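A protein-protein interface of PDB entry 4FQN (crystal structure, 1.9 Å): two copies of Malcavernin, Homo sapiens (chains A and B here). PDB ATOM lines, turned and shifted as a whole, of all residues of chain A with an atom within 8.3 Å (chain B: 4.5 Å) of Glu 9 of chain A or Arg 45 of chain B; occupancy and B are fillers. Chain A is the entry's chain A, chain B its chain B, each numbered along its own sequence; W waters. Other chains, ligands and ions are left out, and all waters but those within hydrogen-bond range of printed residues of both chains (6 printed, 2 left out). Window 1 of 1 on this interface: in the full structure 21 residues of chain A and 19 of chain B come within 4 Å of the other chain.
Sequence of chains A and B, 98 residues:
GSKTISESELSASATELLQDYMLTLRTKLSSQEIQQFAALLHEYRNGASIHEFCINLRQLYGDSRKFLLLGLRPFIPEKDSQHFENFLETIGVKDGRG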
ATOM      1  N   GLY A   1      -1.807  18.284  -1.171  1.00  0.00           N
ATOM      2  CA  GLY A   1      -0.624  17.839  -1.880  1.00  0.00           C
ATOM      3  C   GLY A   1      -0.085  16.525  -1.349  1.00  0.00           C
ATOM      4  O   GLY A   1      -0.658  15.920  -0.448  1.00  0.00           O
ATOM      5  N   SER A   2       1.036  16.085  -1.900  1.00  0.00           N
ATOM      6  CA  SER A   2       1.588  14.813  -1.507  1.00  0.00           C
ATOM      7  C   SER A   2       2.006  14.805  -0.038  1.00  0.00           C
ATOM      8  O   SER A   2       2.032  13.753   0.575  1.00  0.00           O
ATOM      9  CB  SER A   2       2.750  14.418  -2.413  1.00  0.00           C
ATOM     10  OG  SER A   2       3.734  15.427  -2.449  1.00  0.00           O
ATOM     11  N   THR A   4       0.313  15.929   2.436  1.00  0.00           N
ATOM     12  CA  THR A   4      -0.870  16.016   3.284  1.00  0.00           C
ATOM     13  C   THR A   4      -1.856  14.920   2.941  1.00  0.00           C
ATOM     14  O   THR A   4      -2.367  14.856   1.822  1.00  0.00           O
ATOM     15  CB  THR A   4      -1.588  17.390   3.137  1.00  0.00           C
ATOM     16  OG1 THR A   4      -0.657  18.457   3.364  1.00  0.00           O
ATOM     17  CG2 THR A   4      -2.736  17.499   4.119  1.00  0.00           C
ATOM     18  N   ILE A   5      -2.103  14.024   3.894  1.00  0.00           N
ATOM     19  CA  ILE A   5      -3.148  13.023   3.728  1.00  0.00           C
ATOM     20  C   ILE A   5      -4.499  13.733   3.831  1.00  0.00           C
ATOM     21  O   ILE A   5      -4.800  14.368   4.858  1.00  0.00           O
ATOM     22  CB  ILE A   5      -3.047  11.921   4.795  1.00  0.00           C
ATOM     23  CG1 ILE A   5      -1.642  11.315   4.801  1.00  0.00           C
ATOM     24  CG2 ILE A   5      -4.081  10.844   4.539  1.00  0.00           C
ATOM     25  CD1 ILE A   5      -1.256  10.680   3.489  1.00  0.00           C
ATOM     26  N   SER A   6      -5.307  13.657   2.773  1.00  0.00           N
ATOM     27  CA  SER A   6      -6.540  14.459   2.707  1.00  0.00           C
ATOM     28  C   SER A   6      -7.677  13.853   3.519  1.00  0.00           C
ATOM     29  O   SER A   6      -7.615  12.695   3.906  1.00  0.00           O
ATOM     30  CB  SER A   6      -7.016  14.614   1.265  1.00  0.00           C
ATOM     31  OG  SER A   6      -7.633  13.402   0.851  1.00  0.00           O
ATOM     32  N   GLU A   7      -8.708  14.662   3.775  1.00  0.00           N
ATOM     33  CA  GLU A   7      -9.876  14.208   4.529  1.00  0.00           C
ATOM     34  C   GLU A   7     -10.438  12.866   4.050  1.00  0.00           C
ATOM     35  O   GLU A   7     -10.712  11.984   4.865  1.00  0.00           O
ATOM     36  CB  GLU A   7     -10.992  15.263   4.523  1.00  0.00           C
ATOM     37  CG  GLU A   7     -12.195  14.873   5.378  1.00  0.00           C
ATOM     38  CD  GLU A   7     -13.244  14.052   4.630  1.00  0.00           C
ATOM     39  OE1 GLU A   7     -13.303  14.137   3.384  1.00  0.00           O
ATOM     40  OE2 GLU A   7     -14.007  13.316   5.290  1.00  0.00           O
ATOM     41  N   SER A   8     -10.611  12.692   2.744  1.00  0.00           N
ATOM     42  CA  SER A   8     -11.232  11.461   2.258  1.00  0.00           C
ATOM     43  C   SER A   8     -10.374  10.216   2.476  1.00  0.00           C
ATOM     44  O   SER A   8     -10.903   9.109   2.615  1.00  0.00           O
ATOM     45  CB  SER A   8     -11.657  11.587   0.790  1.00  0.00           C
ATOM     46  OG  SER A   8     -10.537  11.626  -0.070  1.00  0.00           O
ATOM     47  N   GLU A   9      -9.057  10.403   2.519  1.00  0.00           N
ATOM     48  CA  GLU A   9      -8.144   9.298   2.780  1.00  0.00           C
ATOM     49  C   GLU A   9      -8.180   8.863   4.244  1.00  0.00           C
ATOM     50  O   GLU A   9      -7.726   7.764   4.584  1.00  0.00           O
ATOM     51  CB  GLU A   9      -6.723   9.689   2.387  1.00  0.00           C
ATOM     52  CG  GLU A   9      -6.314   9.190   1.021  1.00  0.00           C
ATOM     53  CD  GLU A   9      -4.829   9.359   0.748  1.00  0.00           C
ATOM     54  OE1 GLU A   9      -4.359  10.506   0.821  1.00  0.00           O
ATOM     55  OE2 GLU A   9      -4.140   8.345   0.461  1.00  0.00           O
ATOM     56  N   LEU A  10      -8.736   9.730   5.096  1.00  0.00           N
ATOM     57  CA  LEU A  10      -8.803   9.512   6.543  1.00  0.00           C
ATOM     58  C   LEU A  10     -10.222   9.241   7.050  1.00  0.00           C
ATOM     59  O   LEU A  10     -10.428   9.009   8.239  1.00  0.00           O
ATOM     60  CB  LEU A  10      -8.266  10.746   7.281  1.00  0.00           C
ATOM     61  CG  LEU A  10      -6.808  11.135   7.057  1.00  0.00           C
ATOM     62  CD1 LEU A  10      -6.542  12.561   7.546  1.00  0.00           C
ATOM     63  CD2 LEU A  10      -5.902  10.128   7.764  1.00  0.00           C
ATOM     64  N   SER A  11     -11.193   9.266   6.147  1.00  0.00           N
ATOM     65  CA  SER A  11     -12.608   9.108   6.498  1.00  0.00           C
ATOM     66  C   SER A  11     -13.140   7.726   6.133  1.00  0.00           C
ATOM     67  O   SER A  11     -13.154   7.371   4.960  1.00  0.00           O
ATOM     68  CB  SER A  11     -13.439  10.159   5.758  1.00  0.00           C
ATOM     69  OG  SER A  11     -14.820   9.839   5.783  1.00  0.00           O
ATOM     70  N   ALA A  12     -13.569   6.946   7.128  1.00  0.00           N
ATOM     71  CA  ALA A  12     -14.148   5.634   6.843  1.00  0.00           C
ATOM     72  C   ALA A  12     -15.367   5.722   5.908  1.00  0.00           C
ATOM     73  O   ALA A  12     -15.543   4.854   5.051  1.00  0.00           O
ATOM     74  CB  ALA A  12     -14.510   4.891   8.142  1.00  0.00           C
ATOM     75  N   ALA A  14     -16.007   7.997   3.558  1.00  0.00           N
ATOM     76  CA  ALA A  14     -15.546   8.226   2.190  1.00  0.00           C
ATOM     77  C   ALA A  14     -14.943   6.947   1.603  1.00  0.00           C
ATOM     78  O   ALA A  14     -15.097   6.669   0.425  1.00  0.00           O
ATOM     79  CB  ALA A  14     -14.544   9.371   2.129  1.00  0.00           C
ATOM     80  N   THR A  15     -14.283   6.153   2.438  1.00  0.00           N
ATOM     81  CA  THR A  15     -13.704   4.912   1.954  1.00  0.00           C
ATOM     82  C   THR A  15     -14.787   3.922   1.514  1.00  0.00           C
ATOM     83  O   THR A  15     -14.643   3.284   0.468  1.00  0.00           O
ATOM     84  CB  THR A  15     -12.735   4.317   2.980  1.00  0.00           C
ATOM     85  OG1 THR A  15     -11.668   5.249   3.188  1.00  0.00           O
ATOM     86  CG2 THR A  15     -12.160   2.982   2.485  1.00  0.00           C
ATOM     87  N   LEU A  18     -15.777   5.038  -1.815  1.00  0.00           N
ATOM     88  CA  LEU A  18     -14.763   4.647  -2.803  1.00  0.00           C
ATOM     89  C   LEU A  18     -14.934   3.191  -3.229  1.00  0.00           C
ATOM     90  O   LEU A  18     -14.953   2.882  -4.424  1.00  0.00           O
ATOM     91  CB  LEU A  18     -13.343   4.894  -2.266  1.00  0.00           C
ATOM     92  CG  LEU A  18     -12.190   4.537  -3.225  1.00  0.00           C
ATOM     93  CD1 LEU A  18     -12.267   5.316  -4.543  1.00  0.00           C
ATOM     94  CD2 LEU A  18     -10.830   4.733  -2.574  1.00  0.00           C
ATOM     95  N   ALA A  38      -7.593   4.249 -11.375  1.00  0.00           N
ATOM     96  CA  ALA A  38      -6.814   4.013 -10.163  1.00  0.00           C
ATOM     97  C   ALA A  38      -5.509   4.805 -10.202  1.00  0.00           C
ATOM     98  O   ALA A  38      -5.096   5.400  -9.200  1.00  0.00           O
ATOM     99  CB  ALA A  38      -6.524   2.521 -10.009  1.00  0.00           C
ATOM    100  N   ALA A  39      -4.852   4.789 -11.361  1.00  0.00           N
ATOM    101  CA  ALA A  39      -3.624   5.551 -11.550  1.00  0.00           C
ATOM    102  C   ALA A  39      -3.881   7.055 -11.356  1.00  0.00           C
ATOM    103  O   ALA A  39      -3.103   7.741 -10.688  1.00  0.00           O
ATOM    104  CB  ALA A  39      -3.027   5.270 -12.930  1.00  0.00           C
ATOM    105  N   LEU A  41      -6.383   8.519  -9.628  1.00  0.00           N
ATOM    106  CA  LEU A  41      -6.703   8.850  -8.248  1.00  0.00           C
ATOM    107  C   LEU A  41      -5.413   8.868  -7.451  1.00  0.00           C
ATOM    108  O   LEU A  41      -5.174   9.766  -6.643  1.00  0.00           O
ATOM    109  CB  LEU A  41      -7.696   7.853  -7.634  1.00  0.00           C
ATOM    110  CG  LEU A  41      -8.023   8.096  -6.154  1.00  0.00           C
ATOM    111  CD1 LEU A  41      -8.669   9.477  -5.905  1.00  0.00           C
ATOM    112  CD2 LEU A  41      -8.910   6.982  -5.593  1.00  0.00           C
ATOM    113  N   HIS A  42      -4.568   7.863  -7.682  1.00  0.00           N
ATOM    114  CA  HIS A  42      -3.276   7.814  -7.001  1.00  0.00           C
ATOM    115  C   HIS A  42      -2.414   9.045  -7.307  1.00  0.00           C
ATOM    116  O   HIS A  42      -1.764   9.576  -6.414  1.00  0.00           O
ATOM    117  CB  HIS A  42      -2.538   6.523  -7.364  1.00  0.00           C
ATOM    118  CG  HIS A  42      -3.007   5.332  -6.592  1.00  0.00           C
ATOM    119  ND1 HIS A  42      -2.895   4.045  -7.061  1.00  0.00           N
ATOM    120  CD2 HIS A  42      -3.575   5.236  -5.363  1.00  0.00           C
ATOM    121  CE1 HIS A  42      -3.376   3.204  -6.160  1.00  0.00           C
ATOM    122  NE2 HIS A  42      -3.782   3.903  -5.119  1.00  0.00           N
ATOM    123  N   GLU A  43      -2.403   9.486  -8.564  1.00  0.00           N
ATOM    124  CA  GLU A  43      -1.638  10.678  -8.948  1.00  0.00           C
ATOM    125  C   GLU A  43      -2.166  11.923  -8.253  1.00  0.00           C
ATOM    126  O   GLU A  43      -1.390  12.734  -7.737  1.00  0.00           O
ATOM    127  CB  GLU A  43      -1.599  10.852 -10.478  1.00  0.00           C
ATOM    128  CG  GLU A  43      -0.612   9.870 -11.125  1.00  0.00           C
ATOM    129  CD  GLU A  43      -0.817   9.675 -12.621  1.00  0.00           C
ATOM    130  OE1 GLU A  43      -1.491  10.506 -13.275  1.00  0.00           O
ATOM    131  OE2 GLU A  43      -0.284   8.674 -13.147  1.00  0.00           O
ATOM    132  N   TYR A  44      -3.486  12.063  -8.222  1.00  0.00           N
ATOM    133  CA  TYR A  44      -4.109  13.183  -7.518  1.00  0.00           C
ATOM    134  C   TYR A  44      -3.746  13.205  -6.041  1.00  0.00           C
ATOM    135  O   TYR A  44      -3.295  14.219  -5.511  1.00  0.00           O
ATOM    136  CB  TYR A  44      -5.630  13.143  -7.684  1.00  0.00           C
ATOM    137  CG  TYR A  44      -6.363  14.279  -7.002  1.00  0.00           C
ATOM    138  CD1 TYR A  44      -5.975  15.598  -7.191  1.00  0.00           C
ATOM    139  CD2 TYR A  44      -7.451  14.032  -6.171  1.00  0.00           C
ATOM    140  CE1 TYR A  44      -6.659  16.644  -6.568  1.00  0.00           C
ATOM    141  CE2 TYR A  44      -8.134  15.066  -5.555  1.00  0.00           C
ATOM    142  CZ  TYR A  44      -7.734  16.369  -5.757  1.00  0.00           C
ATOM    143  OH  TYR A  44      -8.412  17.395  -5.133  1.00  0.00           O
ATOM    144  N   ARG A  45      -3.953  12.084  -5.364  1.00  0.00           N
ATOM    145  CA  ARG A  45      -3.596  11.983  -3.951  1.00  0.00           C
ATOM    146  C   ARG A  45      -2.100  12.188  -3.732  1.00  0.00           C
ATOM    147  O   ARG A  45      -1.669  12.634  -2.660  1.00  0.00           O
ATOM    148  CB  ARG A  45      -4.104  10.658  -3.380  1.00  0.00           C
ATOM    149  CG  ARG A  45      -5.626  10.683  -3.205  1.00  0.00           C
ATOM    150  CD  ARG A  45      -6.234   9.333  -2.875  1.00  0.00           C
ATOM    151  NE  ARG A  45      -7.556   9.510  -2.284  1.00  0.00           N
ATOM    152  CZ  ARG A  45      -8.262   8.535  -1.728  1.00  0.00           C
ATOM    153  NH1 ARG A  45      -7.780   7.293  -1.692  1.00  0.00           N
ATOM    154  NH2 ARG A  45      -9.449   8.805  -1.197  1.00  0.00           N
ATOM    155  N   ASN A  46      -1.315  11.915  -4.774  1.00  0.00           N
ATOM    156  CA  ASN A  46       0.125  12.143  -4.728  1.00  0.00           C
ATOM    157  C   ASN A  46       0.530  13.537  -5.206  1.00  0.00           C
ATOM    158  O   ASN A  46       1.708  13.797  -5.432  1.00  0.00           O
ATOM    159  CB  ASN A  46       0.875  11.098  -5.560  1.00  0.00           C
ATOM    160  CG  ASN A  46       2.330  10.970  -5.162  1.00  0.00           C
ATOM    161  OD1 ASN A  46       2.679  11.071  -3.977  1.00  0.00           O
ATOM    162  ND2 ASN A  46       3.202  10.756  -6.155  1.00  0.00           N
ATOM    163  N   PRO A  74     -16.963  12.926  -2.982  1.00  0.00           N
ATOM    164  CA  PRO A  74     -16.415  12.712  -1.632  1.00  0.00           C
ATOM    165  C   PRO A  74     -14.887  12.645  -1.521  1.00  0.00           C
ATOM    166  O   PRO A  74     -14.390  12.676  -0.396  1.00  0.00           O
ATOM    167  CB  PRO A  74     -17.013  11.362  -1.223  1.00  0.00           C
ATOM    168  CG  PRO A  74     -18.239  11.232  -2.027  1.00  0.00           C
ATOM    169  CD  PRO A  74     -17.891  11.846  -3.360  1.00  0.00           C
ATOM    170  N   PHE A  75     -14.168  12.567  -2.637  1.00  0.00           N
ATOM    171  CA  PHE A  75     -12.725  12.335  -2.601  1.00  0.00           C
ATOM    172  C   PHE A  75     -11.947  13.615  -2.865  1.00  0.00           C
ATOM    173  O   PHE A  75     -10.709  13.619  -2.876  1.00  0.00           O
ATOM    174  CB  PHE A  75     -12.358  11.218  -3.586  1.00  0.00           C
ATOM    175  CG  PHE A  75     -13.300  10.044  -3.504  1.00  0.00           C
ATOM    176  CD1 PHE A  75     -13.447   9.356  -2.314  1.00  0.00           C
ATOM    177  CD2 PHE A  75     -14.076   9.670  -4.593  1.00  0.00           C
ATOM    178  CE1 PHE A  75     -14.343   8.304  -2.212  1.00  0.00           C
ATOM    179  CE2 PHE A  75     -14.972   8.607  -4.504  1.00  0.00           C
ATOM    180  CZ  PHE A  75     -15.114   7.938  -3.317  1.00  0.00           C
ATOM    181  N   ILE A  76     -12.690  14.706  -3.036  1.00  0.00           N
ATOM    182  CA  ILE A  76     -12.116  16.017  -3.307  1.00  0.00           C
ATOM    183  C   ILE A  76     -12.076  16.826  -2.011  1.00  0.00           C
ATOM    184  O   ILE A  76     -13.116  17.181  -1.455  1.00  0.00           O
ATOM    185  CB  ILE A  76     -12.936  16.771  -4.380  1.00  0.00           C
ATOM    186  CG1 ILE A  76     -13.185  15.864  -5.595  1.00  0.00           C
ATOM    187  CG2 ILE A  76     -12.246  18.068  -4.791  1.00  0.00           C
ATOM    188  CD1 ILE A  76     -11.908  15.275  -6.222  1.00  0.00           C
ATOM    189  N   PRO A  77     -10.868  17.111  -1.515  1.00  0.00           N
ATOM    190  CA  PRO A  77     -10.769  17.892  -0.281  1.00  0.00           C
ATOM    191  C   PRO A  77     -11.300  19.319  -0.486  1.00  0.00           C
ATOM    192  O   PRO A  77     -11.507  19.762  -1.619  1.00  0.00           O
ATOM    193  CB  PRO A  77      -9.271  17.907   0.001  1.00  0.00           C
ATOM    194  CG  PRO A  77      -8.639  17.751  -1.335  1.00  0.00           C
ATOM    195  CD  PRO A  77      -9.551  16.842  -2.112  1.00  0.00           C
ATOM    196  N   SER B   2       2.293  -0.660  -7.692  1.00  0.00           N
ATOM    197  CA  SER B   2       1.250  -0.389  -6.714  1.00  0.00           C
ATOM    198  C   SER B   2       0.105   0.390  -7.359  1.00  0.00           C
ATOM    199  O   SER B   2      -0.560   1.175  -6.702  1.00  0.00           O
ATOM    200  CB  SER B   2       1.813   0.394  -5.516  1.00  0.00           C
ATOM    201  OG  SER B   2       2.918  -0.260  -4.893  1.00  0.00           O
ATOM    202  N   GLU B   9      -6.715   0.279   0.826  1.00  0.00           N
ATOM    203  CA  GLU B   9      -7.285   1.553   0.423  1.00  0.00           C
ATOM    204  C   GLU B   9      -8.811   1.530   0.288  1.00  0.00           C
ATOM    205  O   GLU B   9      -9.452   2.583   0.333  1.00  0.00           O
ATOM    206  CB  GLU B   9      -6.666   2.042  -0.896  1.00  0.00           C
ATOM    207  CG  GLU B   9      -5.182   2.333  -0.827  1.00  0.00           C
ATOM    208  CD  GLU B   9      -4.552   2.421  -2.214  1.00  0.00           C
ATOM    209  OE1 GLU B   9      -4.904   3.371  -2.955  1.00  0.00           O
ATOM    210  OE2 GLU B   9      -3.725   1.530  -2.564  1.00  0.00           O
ATOM    211  N   THR B  15      -8.967   2.593   6.942  1.00  0.00           N
ATOM    212  CA  THR B  15      -8.978   4.051   6.946  1.00  0.00           C
ATOM    213  C   THR B  15      -9.168   4.594   8.348  1.00  0.00           C
ATOM    214  O   THR B  15      -8.485   5.543   8.745  1.00  0.00           O
ATOM    215  CB  THR B  15     -10.064   4.582   6.024  1.00  0.00           C
ATOM    216  OG1 THR B  15      -9.750   4.180   4.689  1.00  0.00           O
ATOM    217  CG2 THR B  15     -10.126   6.114   6.083  1.00  0.00           C
ATOM    218  N   LEU B  18      -5.938   4.403   9.997  1.00  0.00           N
ATOM    219  CA  LEU B  18      -4.987   5.401   9.513  1.00  0.00           C
ATOM    220  C   LEU B  18      -5.208   6.712  10.260  1.00  0.00           C
ATOM    221  O   LEU B  18      -4.249   7.331  10.735  1.00  0.00           O
ATOM    222  CB  LEU B  18      -5.097   5.600   7.989  1.00  0.00           C
ATOM    223  CG  LEU B  18      -4.155   6.638   7.368  1.00  0.00           C
ATOM    224  CD1 LEU B  18      -2.673   6.337   7.642  1.00  0.00           C
ATOM    225  CD2 LEU B  18      -4.404   6.742   5.868  1.00  0.00           C
ATOM    226  N   LEU B  41       3.690   7.557   2.216  1.00  0.00           N
ATOM    227  CA  LEU B  41       2.514   6.709   2.077  1.00  0.00           C
ATOM    228  C   LEU B  41       1.914   6.956   0.693  1.00  0.00           C
ATOM    229  O   LEU B  41       1.502   6.018   0.011  1.00  0.00           O
ATOM    230  CB  LEU B  41       1.474   6.992   3.166  1.00  0.00           C
ATOM    231  CG  LEU B  41       0.183   6.169   3.091  1.00  0.00           C
ATOM    232  CD1 LEU B  41       0.465   4.663   3.180  1.00  0.00           C
ATOM    233  CD2 LEU B  41      -0.869   6.614   4.152  1.00  0.00           C
ATOM    234  N   HIS B  42       1.898   8.218   0.275  1.00  0.00           N
ATOM    235  CA  HIS B  42       1.356   8.568  -1.038  1.00  0.00           C
ATOM    236  C   HIS B  42       2.207   7.964  -2.158  1.00  0.00           C
ATOM    237  O   HIS B  42       1.673   7.486  -3.158  1.00  0.00           O
ATOM    238  CB  HIS B  42       1.240  10.087  -1.199  1.00  0.00           C
ATOM    239  CG  HIS B  42       0.038  10.680  -0.512  1.00  0.00           C
ATOM    240  ND1 HIS B  42       0.027  11.977  -0.035  1.00  0.00           N
ATOM    241  CD2 HIS B  42      -1.190  10.175  -0.273  1.00  0.00           C
ATOM    242  CE1 HIS B  42      -1.165  12.233   0.484  1.00  0.00           C
ATOM    243  NE2 HIS B  42      -1.922  11.161   0.357  1.00  0.00           N
ATOM    244  N   GLU B  43       3.523   7.985  -1.994  1.00  0.00           N
ATOM    245  CA  GLU B  43       4.402   7.410  -3.004  1.00  0.00           C
ATOM    246  C   GLU B  43       4.266   5.884  -3.050  1.00  0.00           C
ATOM    247  O   GLU B  43       4.272   5.294  -4.129  1.00  0.00           O
ATOM    248  CB  GLU B  43       5.858   7.848  -2.803  1.00  0.00           C
ATOM    249  CG  GLU B  43       6.131   9.295  -3.218  1.00  0.00           C
ATOM    250  CD  GLU B  43       6.234   9.482  -4.729  1.00  0.00           C
ATOM    251  OE1 GLU B  43       6.347   8.470  -5.456  1.00  0.00           O
ATOM    252  OE2 GLU B  43       6.222  10.649  -5.194  1.00  0.00           O
ATOM    253  N   TYR B  44       4.128   5.257  -1.883  1.00  0.00           N
ATOM    254  CA  TYR B  44       3.884   3.811  -1.817  1.00  0.00           C
ATOM    255  C   TYR B  44       2.579   3.456  -2.513  1.00  0.00           C
ATOM    256  O   TYR B  44       2.522   2.543  -3.342  1.00  0.00           O
ATOM    257  CB  TYR B  44       3.825   3.347  -0.355  1.00  0.00           C
ATOM    258  CG  TYR B  44       3.403   1.902  -0.173  1.00  0.00           C
ATOM    259  CD1 TYR B  44       4.078   0.880  -0.818  1.00  0.00           C
ATOM    260  CD2 TYR B  44       2.337   1.566   0.659  1.00  0.00           C
ATOM    261  CE1 TYR B  44       3.701  -0.444  -0.643  1.00  0.00           C
ATOM    262  CE2 TYR B  44       1.955   0.249   0.845  1.00  0.00           C
ATOM    263  CZ  TYR B  44       2.638  -0.751   0.182  1.00  0.00           C
ATOM    264  OH  TYR B  44       2.268  -2.068   0.360  1.00  0.00           O
ATOM    265  N   ARG B  45       1.516   4.165  -2.152  1.00  0.00           N
ATOM    266  CA  ARG B  45       0.248   3.960  -2.815  1.00  0.00           C
ATOM    267  C   ARG B  45       0.309   4.240  -4.316  1.00  0.00           C
ATOM    268  O   ARG B  45      -0.371   3.567  -5.077  1.00  0.00           O
ATOM    269  CB  ARG B  45      -0.870   4.755  -2.129  1.00  0.00           C
ATOM    270  CG  ARG B  45      -1.270   4.107  -0.797  1.00  0.00           C
ATOM    271  CD  ARG B  45      -2.288   4.911  -0.002  1.00  0.00           C
ATOM    272  NE  ARG B  45      -2.777   4.109   1.120  1.00  0.00           N
ATOM    273  CZ  ARG B  45      -3.788   4.450   1.907  1.00  0.00           C
ATOM    274  NH1 ARG B  45      -4.427   5.599   1.721  1.00  0.00           N
ATOM    275  NH2 ARG B  45      -4.166   3.635   2.882  1.00  0.00           N
ATOM    276  N   ASN B  46       1.135   5.197  -4.744  1.00  0.00           N
ATOM    277  CA  ASN B  46       1.218   5.538  -6.166  1.00  0.00           C
ATOM    278  C   ASN B  46       2.086   4.563  -6.978  1.00  0.00           C
ATOM    279  O   ASN B  46       1.906   4.417  -8.187  1.00  0.00           O
ATOM    280  CB  ASN B  46       1.696   6.983  -6.365  1.00  0.00           C
ATOM    281  CG  ASN B  46       1.629   7.436  -7.826  1.00  0.00           C
ATOM    282  OD1 ASN B  46       0.612   7.281  -8.490  1.00  0.00           O
ATOM    283  ND2 ASN B  46       2.726   7.994  -8.326  1.00  0.00           N
ATOM    284  N   GLY B  47       3.015   3.879  -6.328  1.00  0.00           N
ATOM    285  CA  GLY B  47       3.846   2.940  -7.066  1.00  0.00           C
ATOM    286  C   GLY B  47       5.185   2.574  -6.452  1.00  0.00           C
ATOM    287  O   GLY B  47       5.875   1.708  -6.981  1.00  0.00           O
HETATM  288  O   HOH W   1      -0.512   4.076  -9.258  1.00  0.00           O
HETATM  289  O   HOH W   2       2.828  11.239  -9.061  1.00  0.00           O
HETATM  290  O   HOH W   3      -8.886   5.205   0.580  1.00  0.00           O
HETATM  291  O   HOH W   4      -1.167   8.180  -3.862  1.00  0.00           O
HETATM  292  O   HOH W   5      -5.450   6.071  -2.568  1.00  0.00           O
HETATM  293  O   HOH W   6      -7.119   5.745   2.944  1.00  0.00           O
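The backbone carbonyl oxygen (O) of Ser 2 of chain A sits at hydrogen-bond distance from a ring nitrogen (ND1) of His 42 of chain B (2.7 Å).
A ring nitrogen (NE2) of His 42 of chain B sits at hydrogen-bond distance from the side-chain carboxylate of Glu 9 of chain A (2.6 Å).
The guanidinium group (NH1) of Arg 45 of chain B lies within salt-bridge range of the side-chain carboxylate (OE2) of Glu 9 of chain A, 3.0 Å away.
The side-chain hydroxyl (OG1) of Thr 15 of chain A sits at hydrogen-bond distance from the side-chain hydroxyl (OG1) of Thr 15 of chain B, 2.7 Å away.
NE2 of His 42 of chain A sits at hydrogen-bond distance from OE1 of Glu 9 of chain B (2.5 Å).
The backbone carbonyl oxygen (O) of Arg 45 of chain B sits close to a ring nitrogen (ND1) of His 42 of chain A (3.2 Å).
The backbone carbonyl oxygen (O) of Arg 45 of chain A sits at hydrogen-bond distance from a ring nitrogen (ND1) of His 42 of chain B.
The side-chain carboxylate (OE2) of Glu 43 of chain B lies within hydrogen-bond range of the side-chain amide nitrogen (ND2) of Asn 46 of chain A, 3.2 Å away.
The backbone carbonyl oxygen (O) of Ala 38 of chain A sits close to a ring nitrogen (ND1) of His 42 of chain A, at 3.4 Å.
The backbone carbonyl oxygen of Tyr 44 of chain B lies close to the side-chain hydroxyl of Ser 2 of chain B (3.2 Å).
Among the printed residues, merely in contact across the chains: Thr 4 of chain A with His 42 of chain B (3.2 Å), Ile 5 of chain A with His 42 of chain B (3.2 Å), Leu 10 of chain A with Thr 15 of chain B (3.3 Å), Glu 9 of chain A with Thr 15 of chain B (3.3 Å), Asn 46 of chain A with His 42 of chain B (3.3 Å), Ser 11 of chain A with Thr 15 of chain B (3.3 Å), His 42 of chain A with Asn 46 of chain B (3.4 Å), Thr 15 of chain A with Glu 9 of chain B (3.5 Å), His 42 of chain A with Ser 2 of chain B (3.5 Å), Asn 46 of chain A with Asn 46 of chain B (3.5 Å), Ala 12 of chain A with Thr 15 of chain B (3.7 Å), Glu 9 of chain A with Leu 18 of chain B (3.7 Å), Glu 43 of chain A with Asn 46 of chain B (3.7 Å), Gly 1 of chain A with His 42 of chain B (3.8 Å), Leu 18 of chain A with Glu 9 of chain B (3.9 Å) and Leu 10 of chain A with Leu 18 of chain B (3.9 Å).
Glu 9 of chain A touches just these residues of chain B: Thr 15 (3.3 Å), Leu 18 (3.7 Å), His 42 (2.6 Å) and Arg 45 (3.0 Å).
Ala 14 of chain A touches none of the printed residues of chain B.
Ile 76 of chain A touches none of the printed residues of chain B.
Of the printed residues of chain A, Thr 15 of chain B touches Glu 9 (3.3 Å), Leu 10 (3.3 Å), Ser 11 (3.3 Å), Ala 12 (3.7 Å) and Thr 15 (2.7 Å).
Printed residues of chain A within 4 Å of Leu 18 of chain B: Glu 9 and Leu 10.
Arg 45 of chain B touches just these residues of chain A: Glu 9 and His 42.
The nearest printed residue of chain B that does not touch Glu 9 of chain A is Leu 41 of chain B (5.2 Å).
The nearest residue of chain A that does not touch Arg 45 of chain B is Arg 45 of chain A (5.1 Å).
Of the 26 printed residues of chain A, 14 touch a printed residue of chain B.
Hydrophobic or aromatic side chains of chain A within 4 Å of the printed part of chain B: Ile 5, Leu 10, Leu 18 and His 42.
Among the printed residues, 24 pairs touch across the chains.
Thr 15 of chain A touches its own counterpart, Thr 15 of chain B.
His 42 of chain A touches Arg 45 of chain B, and with the chains exchanged Arg 45 of chain A touches His 42 of chain B.
His 42 of chain A touches Asn 46 of chain B, and with the chains exchanged Asn 46 of chain A touches His 42 of chain B.
Asn 46 of chain B touches its own counterpart, Asn 46 of chain A.
Water W1 bridges the backbone carbonyl oxygen (O) of Asn 46 of chain B and a ring nitrogen (ND1) of His 42 of chain A.
Water W6 bridges O of Glu 9 of chain A and NH1 of Arg 45 of chain B.
Water W2 bridges the side-chain amide nitrogen of Asn 46 of chain A (3.0 Å) and the side-chain amide nitrogen of Asn 46 of chain B (3.3 Å).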
